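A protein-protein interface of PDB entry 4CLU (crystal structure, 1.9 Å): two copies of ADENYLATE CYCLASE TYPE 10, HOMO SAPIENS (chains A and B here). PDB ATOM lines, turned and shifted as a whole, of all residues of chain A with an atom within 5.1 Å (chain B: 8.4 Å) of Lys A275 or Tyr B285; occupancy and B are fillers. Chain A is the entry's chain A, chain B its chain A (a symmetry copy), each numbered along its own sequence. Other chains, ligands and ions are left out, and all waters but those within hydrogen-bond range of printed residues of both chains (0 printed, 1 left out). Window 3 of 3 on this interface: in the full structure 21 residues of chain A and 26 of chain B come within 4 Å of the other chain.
The backbone carbonyl oxygen of Leu B282 lies close to the side-chain amide oxygen of Gln B276 (3.3 Å).
O of Ser A272 sits at hydrogen-bond distance from NE2 of Gln A281 (3.1 Å).
The backbone carbonyl oxygen (O) of Lys A275 sits at hydrogen-bond distance from the backbone NH (N) of Lys A280, 3.0 Å away.
The backbone NH (N) of Glu B288 sits at hydrogen-bond distance from the backbone carbonyl oxygen (O) of Cys B393 (2.9 Å).
The side-chain amide nitrogen (NE2) of Gln A281 lies within hydrogen-bond range of the side-chain amide oxygen (OE1) of Gln A276 (2.7 Å).
O of Lys A280 sits at hydrogen-bond distance from OH of Tyr B285 (3.2 Å).
NZ of Lys A280 lies within salt-bridge range of OE2 of Glu B69, at 2.8 Å.
The backbone carbonyl oxygen of Gly B284 sits at hydrogen-bond distance from the side-chain amino group of Lys A280 (2.6 Å).
NZ of Lys A280 lies within salt-bridge range of OE2 of Glu B288 (3.8 Å).
The side-chain carboxylate (OD2) of Asp A278 lies within salt-bridge range of the guanidinium group (NE) of Arg B66.
The backbone NH (N) of Gly B284 is in hydrogen-bond range of the backbone carbonyl oxygen (O) of Asn A279 (2.7 Å).
Of chain B, only Tyr B285 (3.96 Å) comes within 4 Å of Lys A275.
Of the printed residues of chain B, Lys A280 touches Glu B69 (2.8 Å), Leu B282 (3.7 Å), Gly B284 (2.6 Å), Tyr B285 (3.2 Å) and Glu B288 (3.7 Å).
Tyr B285 touches two residues of chain A.
Of the printed residues of chain A, Glu B288 touches Lys A280 (3.7 Å).
The nearest residue of chain B that does not touch Lys A275 is Arg B66 (6.2 Å).
The nearest residue of chain A that does not touch Tyr B285 is Asn A279 (4.5 Å).
Among the printed residues, pairs that only touch across the chains: Lys A275 with Tyr B285 (3.96 Å), Asp A278 with Glu B69 (3.6 Å), Asp A278 with Gly B284 (3.1 Å), Asn A279 with Leu B282 (3.3 Å), Asn A279 with Gln B283 (3.7 Å), Lys A280 with Leu B282 (3.7 Å) and Gln A281 with Leu B282 (3.9 Å).
Positions printed for both chains: 272, 276 and 281.
Of the 13 pairs that touch across the chains among the printed residues, none has its exchanged pair printed and touching as well.
Of the 20 printed residues of chain B, 7 touch a printed residue of chain A.
Printed residues of chain B that touch a printed residue of chain A: Arg B66, Glu B69, Leu B282, Gln B283, Gly B284, Tyr B285 and Glu B288.
Hydrophobic or aromatic side chains of chain B within 4 Å of the printed part of chain A: Leu B282 and Tyr B285.
Of the 11 printed residues of chain A, 5 touch a printed residue of chain B.
Among the printed residues, Asp or Glu carboxylates within 4 Å of a Lys or Arg side-chain nitrogen of the other chain: Asp A278 with Arg B66, Lys A280 with Glu B69 and Lys A280 with Glu B288.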
ATOM      1  N   GLU A 271      23.006  10.699  32.812  1.00  0.00           N
ATOM      2  CA  GLU A 271      23.319   9.822  31.656  1.00  0.00           C
ATOM      3  C   GLU A 271      23.383   8.365  31.982  1.00  0.00           C
ATOM      4  O   GLU A 271      22.951   7.515  31.241  1.00  0.00           O
ATOM      5  CB  GLU A 271      24.722  10.111  31.119  1.00  0.00           C
ATOM      6  CG  GLU A 271      24.874  11.508  30.612  1.00  0.00           C
ATOM      7  CD  GLU A 271      24.129  11.714  29.320  1.00  0.00           C
ATOM      8  OE1 GLU A 271      23.767  10.698  28.658  1.00  0.00           O
ATOM      9  OE2 GLU A 271      23.930  12.900  28.987  1.00  0.00           O
ATOM     10  N   SER A 272      24.003   8.054  33.108  1.00  0.00           N
ATOM     11  CA  SER A 272      24.137   6.685  33.503  1.00  0.00           C
ATOM     12  C   SER A 272      22.836   6.006  33.757  1.00  0.00           C
ATOM     13  O   SER A 272      22.718   4.783  33.567  1.00  0.00           O
ATOM     14  CB  SER A 272      25.089   6.579  34.737  1.00  0.00           C
ATOM     15  OG  SER A 272      24.676   7.450  35.769  1.00  0.00           O
ATOM     16  N   ILE A 273      21.806   6.766  34.180  1.00  0.00           N
ATOM     17  CA  ILE A 273      20.490   6.191  34.419  1.00  0.00           C
ATOM     18  C   ILE A 273      19.766   6.002  33.066  1.00  0.00           C
ATOM     19  O   ILE A 273      19.140   5.004  32.837  1.00  0.00           O
ATOM     20  CB  ILE A 273      19.661   7.141  35.313  1.00  0.00           C
ATOM     21  CG1 ILE A 273      20.219   7.133  36.733  1.00  0.00           C
ATOM     22  CG2 ILE A 273      18.185   6.776  35.211  1.00  0.00           C
ATOM     23  CD1 ILE A 273      19.975   5.830  37.465  1.00  0.00           C
ATOM     24  N   LEU A 274      19.948   6.964  32.156  1.00  0.00           N
ATOM     25  CA  LEU A 274      19.422   6.814  30.798  1.00  0.00           C
ATOM     26  C   LEU A 274      20.023   5.576  30.135  1.00  0.00           C
ATOM     27  O   LEU A 274      19.315   4.841  29.488  1.00  0.00           O
ATOM     28  CB  LEU A 274      19.692   8.082  29.974  1.00  0.00           C
ATOM     29  CG  LEU A 274      18.839   9.261  30.398  1.00  0.00           C
ATOM     30  CD1 LEU A 274      19.350  10.478  29.656  1.00  0.00           C
ATOM     31  CD2 LEU A 274      17.297   9.095  30.165  1.00  0.00           C
ATOM     32  N   LYS A 275      21.322   5.323  30.330  1.00  0.00           N
ATOM     33  CA  LYS A 275      21.922   4.098  29.800  1.00  0.00           C
ATOM     34  C   LYS A 275      21.204   2.847  30.292  1.00  0.00           C
ATOM     35  O   LYS A 275      20.911   1.930  29.542  1.00  0.00           O
ATOM     36  CB  LYS A 275      23.396   4.084  30.232  1.00  0.00           C
ATOM     37  CG  LYS A 275      24.270   3.429  29.214  1.00  0.00           C
ATOM     38  CD  LYS A 275      25.750   3.430  29.657  1.00  0.00           C
ATOM     39  CE  LYS A 275      26.447   2.361  28.799  1.00  0.00           C
ATOM     40  NZ  LYS A 275      27.911   2.371  29.012  1.00  0.00           N
ATOM     41  N   GLN A 276      20.914   2.805  31.581  1.00  0.00           N
ATOM     42  CA  GLN A 276      20.164   1.653  32.100  1.00  0.00           C
ATOM     43  C   GLN A 276      18.784   1.504  31.586  1.00  0.00           C
ATOM     44  O   GLN A 276      18.327   0.443  31.225  1.00  0.00           O
ATOM     45  CB  GLN A 276      20.057   1.802  33.581  1.00  0.00           C
ATOM     46  CG  GLN A 276      19.786   0.448  34.154  1.00  0.00           C
ATOM     47  CD  GLN A 276      20.674   0.318  35.366  1.00  0.00           C
ATOM     48  OE1 GLN A 276      21.943   0.205  35.283  1.00  0.00           O
ATOM     49  NE2 GLN A 276      20.035   0.521  36.511  1.00  0.00           N
ATOM     50  N   ILE A 277      18.071   2.620  31.566  1.00  0.00           N
ATOM     51  CA  ILE A 277      16.719   2.674  30.916  1.00  0.00           C
ATOM     52  C   ILE A 277      16.734   2.157  29.527  1.00  0.00           C
ATOM     53  O   ILE A 277      15.795   1.441  29.096  1.00  0.00           O
ATOM     54  CB  ILE A 277      16.229   4.152  30.988  1.00  0.00           C
ATOM     55  CG1 ILE A 277      15.780   4.464  32.431  1.00  0.00           C
ATOM     56  CG2 ILE A 277      15.072   4.417  30.056  1.00  0.00           C
ATOM     57  CD1 ILE A 277      15.453   5.918  32.703  1.00  0.00           C
ATOM     58  N   ASP A 278      17.781   2.549  28.784  1.00  0.00           N
ATOM     59  CA  ASP A 278      17.933   2.136  27.435  1.00  0.00           C
ATOM     60  C   ASP A 278      18.548   0.695  27.266  1.00  0.00           C
ATOM     61  O   ASP A 278      18.825   0.261  26.143  1.00  0.00           O
ATOM     62  CB  ASP A 278      18.824   3.118  26.678  1.00  0.00           C
ATOM     63  CG  ASP A 278      18.122   4.476  26.390  1.00  0.00           C
ATOM     64  OD1 ASP A 278      16.879   4.479  26.303  1.00  0.00           O
ATOM     65  OD2 ASP A 278      18.844   5.465  26.199  1.00  0.00           O
ATOM     66  N   ASN A 279      18.665  -0.044  28.351  1.00  0.00           N
ATOM     67  CA  ASN A 279      19.127  -1.457  28.300  1.00  0.00           C
ATOM     68  C   ASN A 279      20.507  -1.571  27.642  1.00  0.00           C
ATOM     69  O   ASN A 279      20.833  -2.556  26.925  1.00  0.00           O
ATOM     70  CB  ASN A 279      18.123  -2.345  27.635  1.00  0.00           C
ATOM     71  CG  ASN A 279      16.750  -2.354  28.315  1.00  0.00           C
ATOM     72  OD1 ASN A 279      16.611  -2.355  29.522  1.00  0.00           O
ATOM     73  ND2 ASN A 279      15.747  -2.431  27.515  1.00  0.00           N
ATOM     74  N   LYS A 280      21.351  -0.605  27.954  1.00  0.00           N
ATOM     75  CA  LYS A 280      22.717  -0.592  27.536  1.00  0.00           C
ATOM     76  C   LYS A 280      23.684  -0.896  28.675  1.00  0.00           C
ATOM     77  O   LYS A 280      24.881  -0.794  28.486  1.00  0.00           O
ATOM     78  CB  LYS A 280      23.075   0.760  26.896  1.00  0.00           C
ATOM     79  CG  LYS A 280      22.412   0.873  25.555  1.00  0.00           C
ATOM     80  CD  LYS A 280      22.851   2.122  24.828  1.00  0.00           C
ATOM     81  CE  LYS A 280      22.539   1.995  23.348  1.00  0.00           C
ATOM     82  NZ  LYS A 280      21.126   1.548  23.083  1.00  0.00           N
ATOM     83  N   GLN A 281      23.168  -1.245  29.855  1.00  0.00           N
ATOM     84  CA  GLN A 281      24.030  -1.645  30.949  1.00  0.00           C
ATOM     85  C   GLN A 281      23.203  -2.577  31.859  1.00  0.00           C
ATOM     86  O   GLN A 281      22.023  -2.443  31.948  1.00  0.00           O
ATOM     87  CB  GLN A 281      24.682  -0.406  31.597  1.00  0.00           C
ATOM     88  CG  GLN A 281      24.626  -0.141  33.080  1.00  0.00           C
ATOM     89  CD  GLN A 281      24.664   1.395  33.374  1.00  0.00           C
ATOM     90  OE1 GLN A 281      25.505   2.134  32.841  1.00  0.00           O
ATOM     91  NE2 GLN A 281      23.714   1.870  34.176  1.00  0.00           N
ATOM     92  N   ARG B  66      20.404  10.088  21.907  1.00  0.00           N
ATOM     93  CA  ARG B  66      19.433   9.015  22.125  1.00  0.00           C
ATOM     94  C   ARG B  66      18.518   8.980  20.938  1.00  0.00           C
ATOM     95  O   ARG B  66      17.435   8.497  21.018  1.00  0.00           O
ATOM     96  CB  ARG B  66      18.635   9.232  23.420  1.00  0.00           C
ATOM     97  CG  ARG B  66      19.467   8.960  24.678  1.00  0.00           C
ATOM     98  CD  ARG B  66      18.675   9.020  25.986  1.00  0.00           C
ATOM     99  NE  ARG B  66      17.704   7.946  26.023  1.00  0.00           N
ATOM    100  CZ  ARG B  66      16.407   8.078  25.809  1.00  0.00           C
ATOM    101  NH1 ARG B  66      15.862   9.285  25.598  1.00  0.00           N
ATOM    102  NH2 ARG B  66      15.648   7.018  25.835  1.00  0.00           N
ATOM    103  N   ALA B  68      18.536   7.005  18.246  1.00  0.00           N
ATOM    104  CA  ALA B  68      18.103   5.654  17.912  1.00  0.00           C
ATOM    105  C   ALA B  68      17.031   5.146  18.827  1.00  0.00           C
ATOM    106  O   ALA B  68      16.050   4.487  18.419  1.00  0.00           O
ATOM    107  CB  ALA B  68      19.274   4.712  17.981  1.00  0.00           C
ATOM    108  N   GLU B  69      17.205   5.434  20.112  1.00  0.00           N
ATOM    109  CA  GLU B  69      16.178   4.999  21.072  1.00  0.00           C
ATOM    110  C   GLU B  69      14.847   5.690  20.901  1.00  0.00           C
ATOM    111  O   GLU B  69      13.774   5.038  20.962  1.00  0.00           O
ATOM    112  CB  GLU B  69      16.679   5.250  22.470  1.00  0.00           C
ATOM    113  CG  GLU B  69      17.917   4.417  22.831  1.00  0.00           C
ATOM    114  CD  GLU B  69      19.248   4.871  22.270  1.00  0.00           C
ATOM    115  OE1 GLU B  69      19.439   5.958  21.701  1.00  0.00           O
ATOM    116  OE2 GLU B  69      20.152   4.031  22.302  1.00  0.00           O
ATOM    117  N   SER B 272      23.112 -12.231  15.208  1.00  0.00           N
ATOM    118  CA  SER B 272      23.066 -11.213  16.211  1.00  0.00           C
ATOM    119  C   SER B 272      21.754 -11.119  16.910  1.00  0.00           C
ATOM    120  O   SER B 272      21.696 -10.727  18.087  1.00  0.00           O
ATOM    121  CB  SER B 272      23.484  -9.840  15.591  1.00  0.00           C
ATOM    122  OG  SER B 272      22.729  -9.558  14.433  1.00  0.00           O
ATOM    123  N   GLN B 276      20.737 -11.999  21.017  1.00  0.00           N
ATOM    124  CA  GLN B 276      19.829 -11.279  21.919  1.00  0.00           C
ATOM    125  C   GLN B 276      18.740 -12.088  22.511  1.00  0.00           C
ATOM    126  O   GLN B 276      18.435 -12.028  23.681  1.00  0.00           O
ATOM    127  CB  GLN B 276      19.177 -10.185  21.142  1.00  0.00           C
ATOM    128  CG  GLN B 276      18.689  -9.164  22.119  1.00  0.00           C
ATOM    129  CD  GLN B 276      19.056  -7.819  21.542  1.00  0.00           C
ATOM    130  OE1 GLN B 276      20.262  -7.406  21.466  1.00  0.00           O
ATOM    131  NE2 GLN B 276      18.038  -7.202  20.956  1.00  0.00           N
ATOM    132  N   GLN B 281      23.409 -10.705  24.972  1.00  0.00           N
ATOM    133  CA  GLN B 281      23.792  -9.336  24.688  1.00  0.00           C
ATOM    134  C   GLN B 281      22.669  -8.430  25.236  1.00  0.00           C
ATOM    135  O   GLN B 281      21.544  -8.819  25.275  1.00  0.00           O
ATOM    136  CB  GLN B 281      24.173  -9.183  23.202  1.00  0.00           C
ATOM    137  CG  GLN B 281      23.570  -8.126  22.313  1.00  0.00           C
ATOM    138  CD  GLN B 281      23.519  -8.609  20.826  1.00  0.00           C
ATOM    139  OE1 GLN B 281      24.510  -9.112  20.276  1.00  0.00           O
ATOM    140  NE2 GLN B 281      22.345  -8.505  20.207  1.00  0.00           N
ATOM    141  N   LEU B 282      23.037  -7.230  25.646  1.00  0.00           N
ATOM    142  CA  LEU B 282      22.095  -6.268  26.213  1.00  0.00           C
ATOM    143  C   LEU B 282      21.165  -5.854  25.095  1.00  0.00           C
ATOM    144  O   LEU B 282      21.638  -5.637  23.941  1.00  0.00           O
ATOM    145  CB  LEU B 282      22.927  -5.121  26.724  1.00  0.00           C
ATOM    146  CG  LEU B 282      23.661  -5.434  28.018  1.00  0.00           C
ATOM    147  CD1 LEU B 282      24.779  -4.488  28.184  1.00  0.00           C
ATOM    148  CD2 LEU B 282      22.690  -5.350  29.173  1.00  0.00           C
ATOM    149  N   GLN B 283      19.869  -5.793  25.390  1.00  0.00           N
ATOM    150  CA  GLN B 283      18.861  -5.352  24.431  1.00  0.00           C
ATOM    151  C   GLN B 283      19.155  -3.999  23.796  1.00  0.00           C
ATOM    152  O   GLN B 283      18.863  -3.805  22.624  1.00  0.00           O
ATOM    153  CB  GLN B 283      17.480  -5.245  25.021  1.00  0.00           C
ATOM    154  CG  GLN B 283      16.911  -6.513  25.586  1.00  0.00           C
ATOM    155  CD  GLN B 283      15.634  -6.235  26.350  1.00  0.00           C
ATOM    156  OE1 GLN B 283      14.573  -6.051  25.735  1.00  0.00           O
ATOM    157  NE2 GLN B 283      15.725  -6.165  27.693  1.00  0.00           N
ATOM    158  N   GLY B 284      19.741  -3.099  24.540  1.00  0.00           N
ATOM    159  CA  GLY B 284      19.961  -1.751  24.051  1.00  0.00           C
ATOM    160  C   GLY B 284      20.759  -1.735  22.763  1.00  0.00           C
ATOM    161  O   GLY B 284      20.659  -0.765  21.983  1.00  0.00           O
ATOM    162  N   TYR B 285      21.594  -2.754  22.541  1.00  0.00           N
ATOM    163  CA  TYR B 285      22.550  -2.635  21.451  1.00  0.00           C
ATOM    164  C   TYR B 285      22.053  -2.939  20.109  1.00  0.00           C
ATOM    165  O   TYR B 285      22.718  -2.586  19.202  1.00  0.00           O
ATOM    166  CB  TYR B 285      23.916  -3.320  21.716  1.00  0.00           C
ATOM    167  CG  TYR B 285      24.636  -2.481  22.765  1.00  0.00           C
ATOM    168  CD1 TYR B 285      25.140  -1.185  22.456  1.00  0.00           C
ATOM    169  CD2 TYR B 285      24.654  -2.889  24.098  1.00  0.00           C
ATOM    170  CE1 TYR B 285      25.725  -0.387  23.427  1.00  0.00           C
ATOM    171  CE2 TYR B 285      25.257  -2.106  25.073  1.00  0.00           C
ATOM    172  CZ  TYR B 285      25.795  -0.882  24.730  1.00  0.00           C
ATOM    173  OH  TYR B 285      26.342  -0.159  25.745  1.00  0.00           O
ATOM    174  N   LEU B 286      20.899  -3.513  19.910  1.00  0.00           N
ATOM    175  CA  LEU B 286      20.489  -3.658  18.493  1.00  0.00           C
ATOM    176  C   LEU B 286      19.770  -2.494  17.848  1.00  0.00           C
ATOM    177  O   LEU B 286      19.661  -2.476  16.631  1.00  0.00           O
ATOM    178  CB  LEU B 286      19.643  -4.863  18.250  1.00  0.00           C
ATOM    179  CG  LEU B 286      20.395  -6.176  18.042  1.00  0.00           C
ATOM    180  CD1 LEU B 286      19.291  -7.222  18.003  1.00  0.00           C
ATOM    181  CD2 LEU B 286      21.294  -6.207  16.817  1.00  0.00           C
ATOM    182  N   SER B 287      19.357  -1.507  18.613  1.00  0.00           N
ATOM    183  CA  SER B 287      18.809  -0.265  18.050  1.00  0.00           C
ATOM    184  C   SER B 287      19.860   0.720  17.946  1.00  0.00           C
ATOM    185  O   SER B 287      20.360   1.217  18.986  1.00  0.00           O
ATOM    186  CB  SER B 287      17.784   0.344  18.994  1.00  0.00           C
ATOM    187  OG  SER B 287      16.730  -0.552  18.935  1.00  0.00           O
ATOM    188  N   GLU B 288      20.271   1.037  16.724  1.00  0.00           N
ATOM    189  CA  GLU B 288      21.394   1.979  16.605  1.00  0.00           C
ATOM    190  C   GLU B 288      21.252   2.821  15.382  1.00  0.00           C
ATOM    191  O   GLU B 288      20.605   2.409  14.418  1.00  0.00           O
ATOM    192  CB  GLU B 288      22.654   1.162  16.421  1.00  0.00           C
ATOM    193  CG  GLU B 288      22.960   0.243  17.609  1.00  0.00           C
ATOM    194  CD  GLU B 288      23.553   0.961  18.824  1.00  0.00           C
ATOM    195  OE1 GLU B 288      24.368   1.890  18.603  1.00  0.00           O
ATOM    196  OE2 GLU B 288      23.228   0.596  20.002  1.00  0.00           O
ATOM    197  N   LEU B 289      21.810   4.012  15.412  1.00  0.00           N
ATOM    198  CA  LEU B 289      21.986   4.774  14.171  1.00  0.00           C
ATOM    199  C   LEU B 289      23.449   4.562  13.857  1.00  0.00           C
ATOM    200  O   LEU B 289      24.300   4.930  14.677  1.00  0.00           O
ATOM    201  CB  LEU B 289      21.679   6.227  14.434  1.00  0.00           C
ATOM    202  CG  LEU B 289      20.232   6.580  14.487  1.00  0.00           C
ATOM    203  CD1 LEU B 289      20.143   7.910  15.119  1.00  0.00           C
ATOM    204  CD2 LEU B 289      19.560   6.625  13.095  1.00  0.00           C
ATOM    205  N   ARG B 290      23.765   3.775  12.833  1.00  0.00           N
ATOM    206  CA  ARG B 290      25.186   3.416  12.628  1.00  0.00           C
ATOM    207  C   ARG B 290      25.579   3.701  11.183  1.00  0.00           C
ATOM    208  O   ARG B 290      24.707   3.744  10.283  1.00  0.00           O
ATOM    209  CB  ARG B 290      25.515   1.990  13.082  1.00  0.00           C
ATOM    210  CG  ARG B 290      24.720   0.874  12.473  1.00  0.00           C
ATOM    211  CD  ARG B 290      24.865  -0.483  13.210  1.00  0.00           C
ATOM    212  NE  ARG B 290      26.217  -1.036  13.012  1.00  0.00           N
ATOM    213  CZ  ARG B 290      27.018  -1.546  13.957  1.00  0.00           C
ATOM    214  NH1 ARG B 290      26.605  -1.696  15.214  1.00  0.00           N
ATOM    215  NH2 ARG B 290      28.245  -1.972  13.632  1.00  0.00           N
ATOM    216  N   PRO B 351      26.011  -5.005  13.251  1.00  0.00           N
ATOM    217  CA  PRO B 351      26.604  -5.528  14.524  1.00  0.00           C
ATOM    218  C   PRO B 351      27.631  -6.651  14.325  1.00  0.00           C
ATOM    219  O   PRO B 351      27.323  -7.671  13.666  1.00  0.00           O
ATOM    220  CB  PRO B 351      25.385  -6.069  15.295  1.00  0.00           C
ATOM    221  CG  PRO B 351      24.191  -5.324  14.736  1.00  0.00           C
ATOM    222  CD  PRO B 351      24.586  -4.646  13.426  1.00  0.00           C
ATOM    223  N   CYS B 393      19.193   0.932  12.291  1.00  0.00           N
ATOM    224  CA  CYS B 393      19.255  -0.533  12.230  1.00  0.00           C
ATOM    225  C   CYS B 393      18.532  -0.950  13.524  1.00  0.00           C
ATOM    226  O   CYS B 393      18.862  -0.402  14.621  1.00  0.00           O
ATOM    227  CB  CYS B 393      20.714  -0.989  12.273  1.00  0.00           C
ATOM    228  SG  CYS B 393      21.660  -0.444  10.854  1.00  0.00           S
ATOM    229  N   GLY B 394      17.438  -1.726  13.424  1.00  0.00           N
ATOM    230  CA  GLY B 394      16.895  -2.216  14.672  1.00  0.00           C
ATOM    231  C   GLY B 394      15.634  -3.035  14.504  1.00  0.00           C
ATOM    232  O   GLY B 394      15.206  -3.254  13.391  1.00  0.00           O
ATOM    233  N   ILE B 395      15.034  -3.405  15.629  1.00  0.00           N
ATOM    234  CA  ILE B 395      13.819  -4.285  15.602  1.00  0.00           C
ATOM    235  C   ILE B 395      12.565  -3.495  15.551  1.00  0.00           C
ATOM    236  O   ILE B 395      12.257  -2.697  16.454  1.00  0.00           O
ATOM    237  CB  ILE B 395      13.846  -5.338  16.764  1.00  0.00           C
ATOM    238  CG1 ILE B 395      14.949  -6.358  16.486  1.00  0.00           C
ATOM    239  CG2 ILE B 395      12.558  -6.181  16.777  1.00  0.00           C
ATOM    240  CD1 ILE B 395      15.419  -7.054  17.748  1.00  0.00           C
ATOM    241  N   TYR B 404      14.220  -7.351  12.432  1.00  0.00           N
ATOM    242  CA  TYR B 404      15.346  -6.437  12.251  1.00  0.00           C
ATOM    243  C   TYR B 404      15.356  -5.858  10.872  1.00  0.00           C
ATOM    244  O   TYR B 404      15.300  -6.554   9.897  1.00  0.00           O
ATOM    245  CB  TYR B 404      16.597  -7.192  12.435  1.00  0.00           C
ATOM    246  CG  TYR B 404      17.827  -6.353  12.609  1.00  0.00           C
ATOM    247  CD1 TYR B 404      18.054  -5.622  13.773  1.00  0.00           C
ATOM    248  CD2 TYR B 404      18.779  -6.317  11.605  1.00  0.00           C
ATOM    249  CE1 TYR B 404      19.255  -4.852  13.946  1.00  0.00           C
ATOM    250  CE2 TYR B 404      19.979  -5.566  11.791  1.00  0.00           C
ATOM    251  CZ  TYR B 404      20.188  -4.849  12.935  1.00  0.00           C
ATOM    252  OH  TYR B 404      21.382  -4.133  13.095  1.00  0.00           O
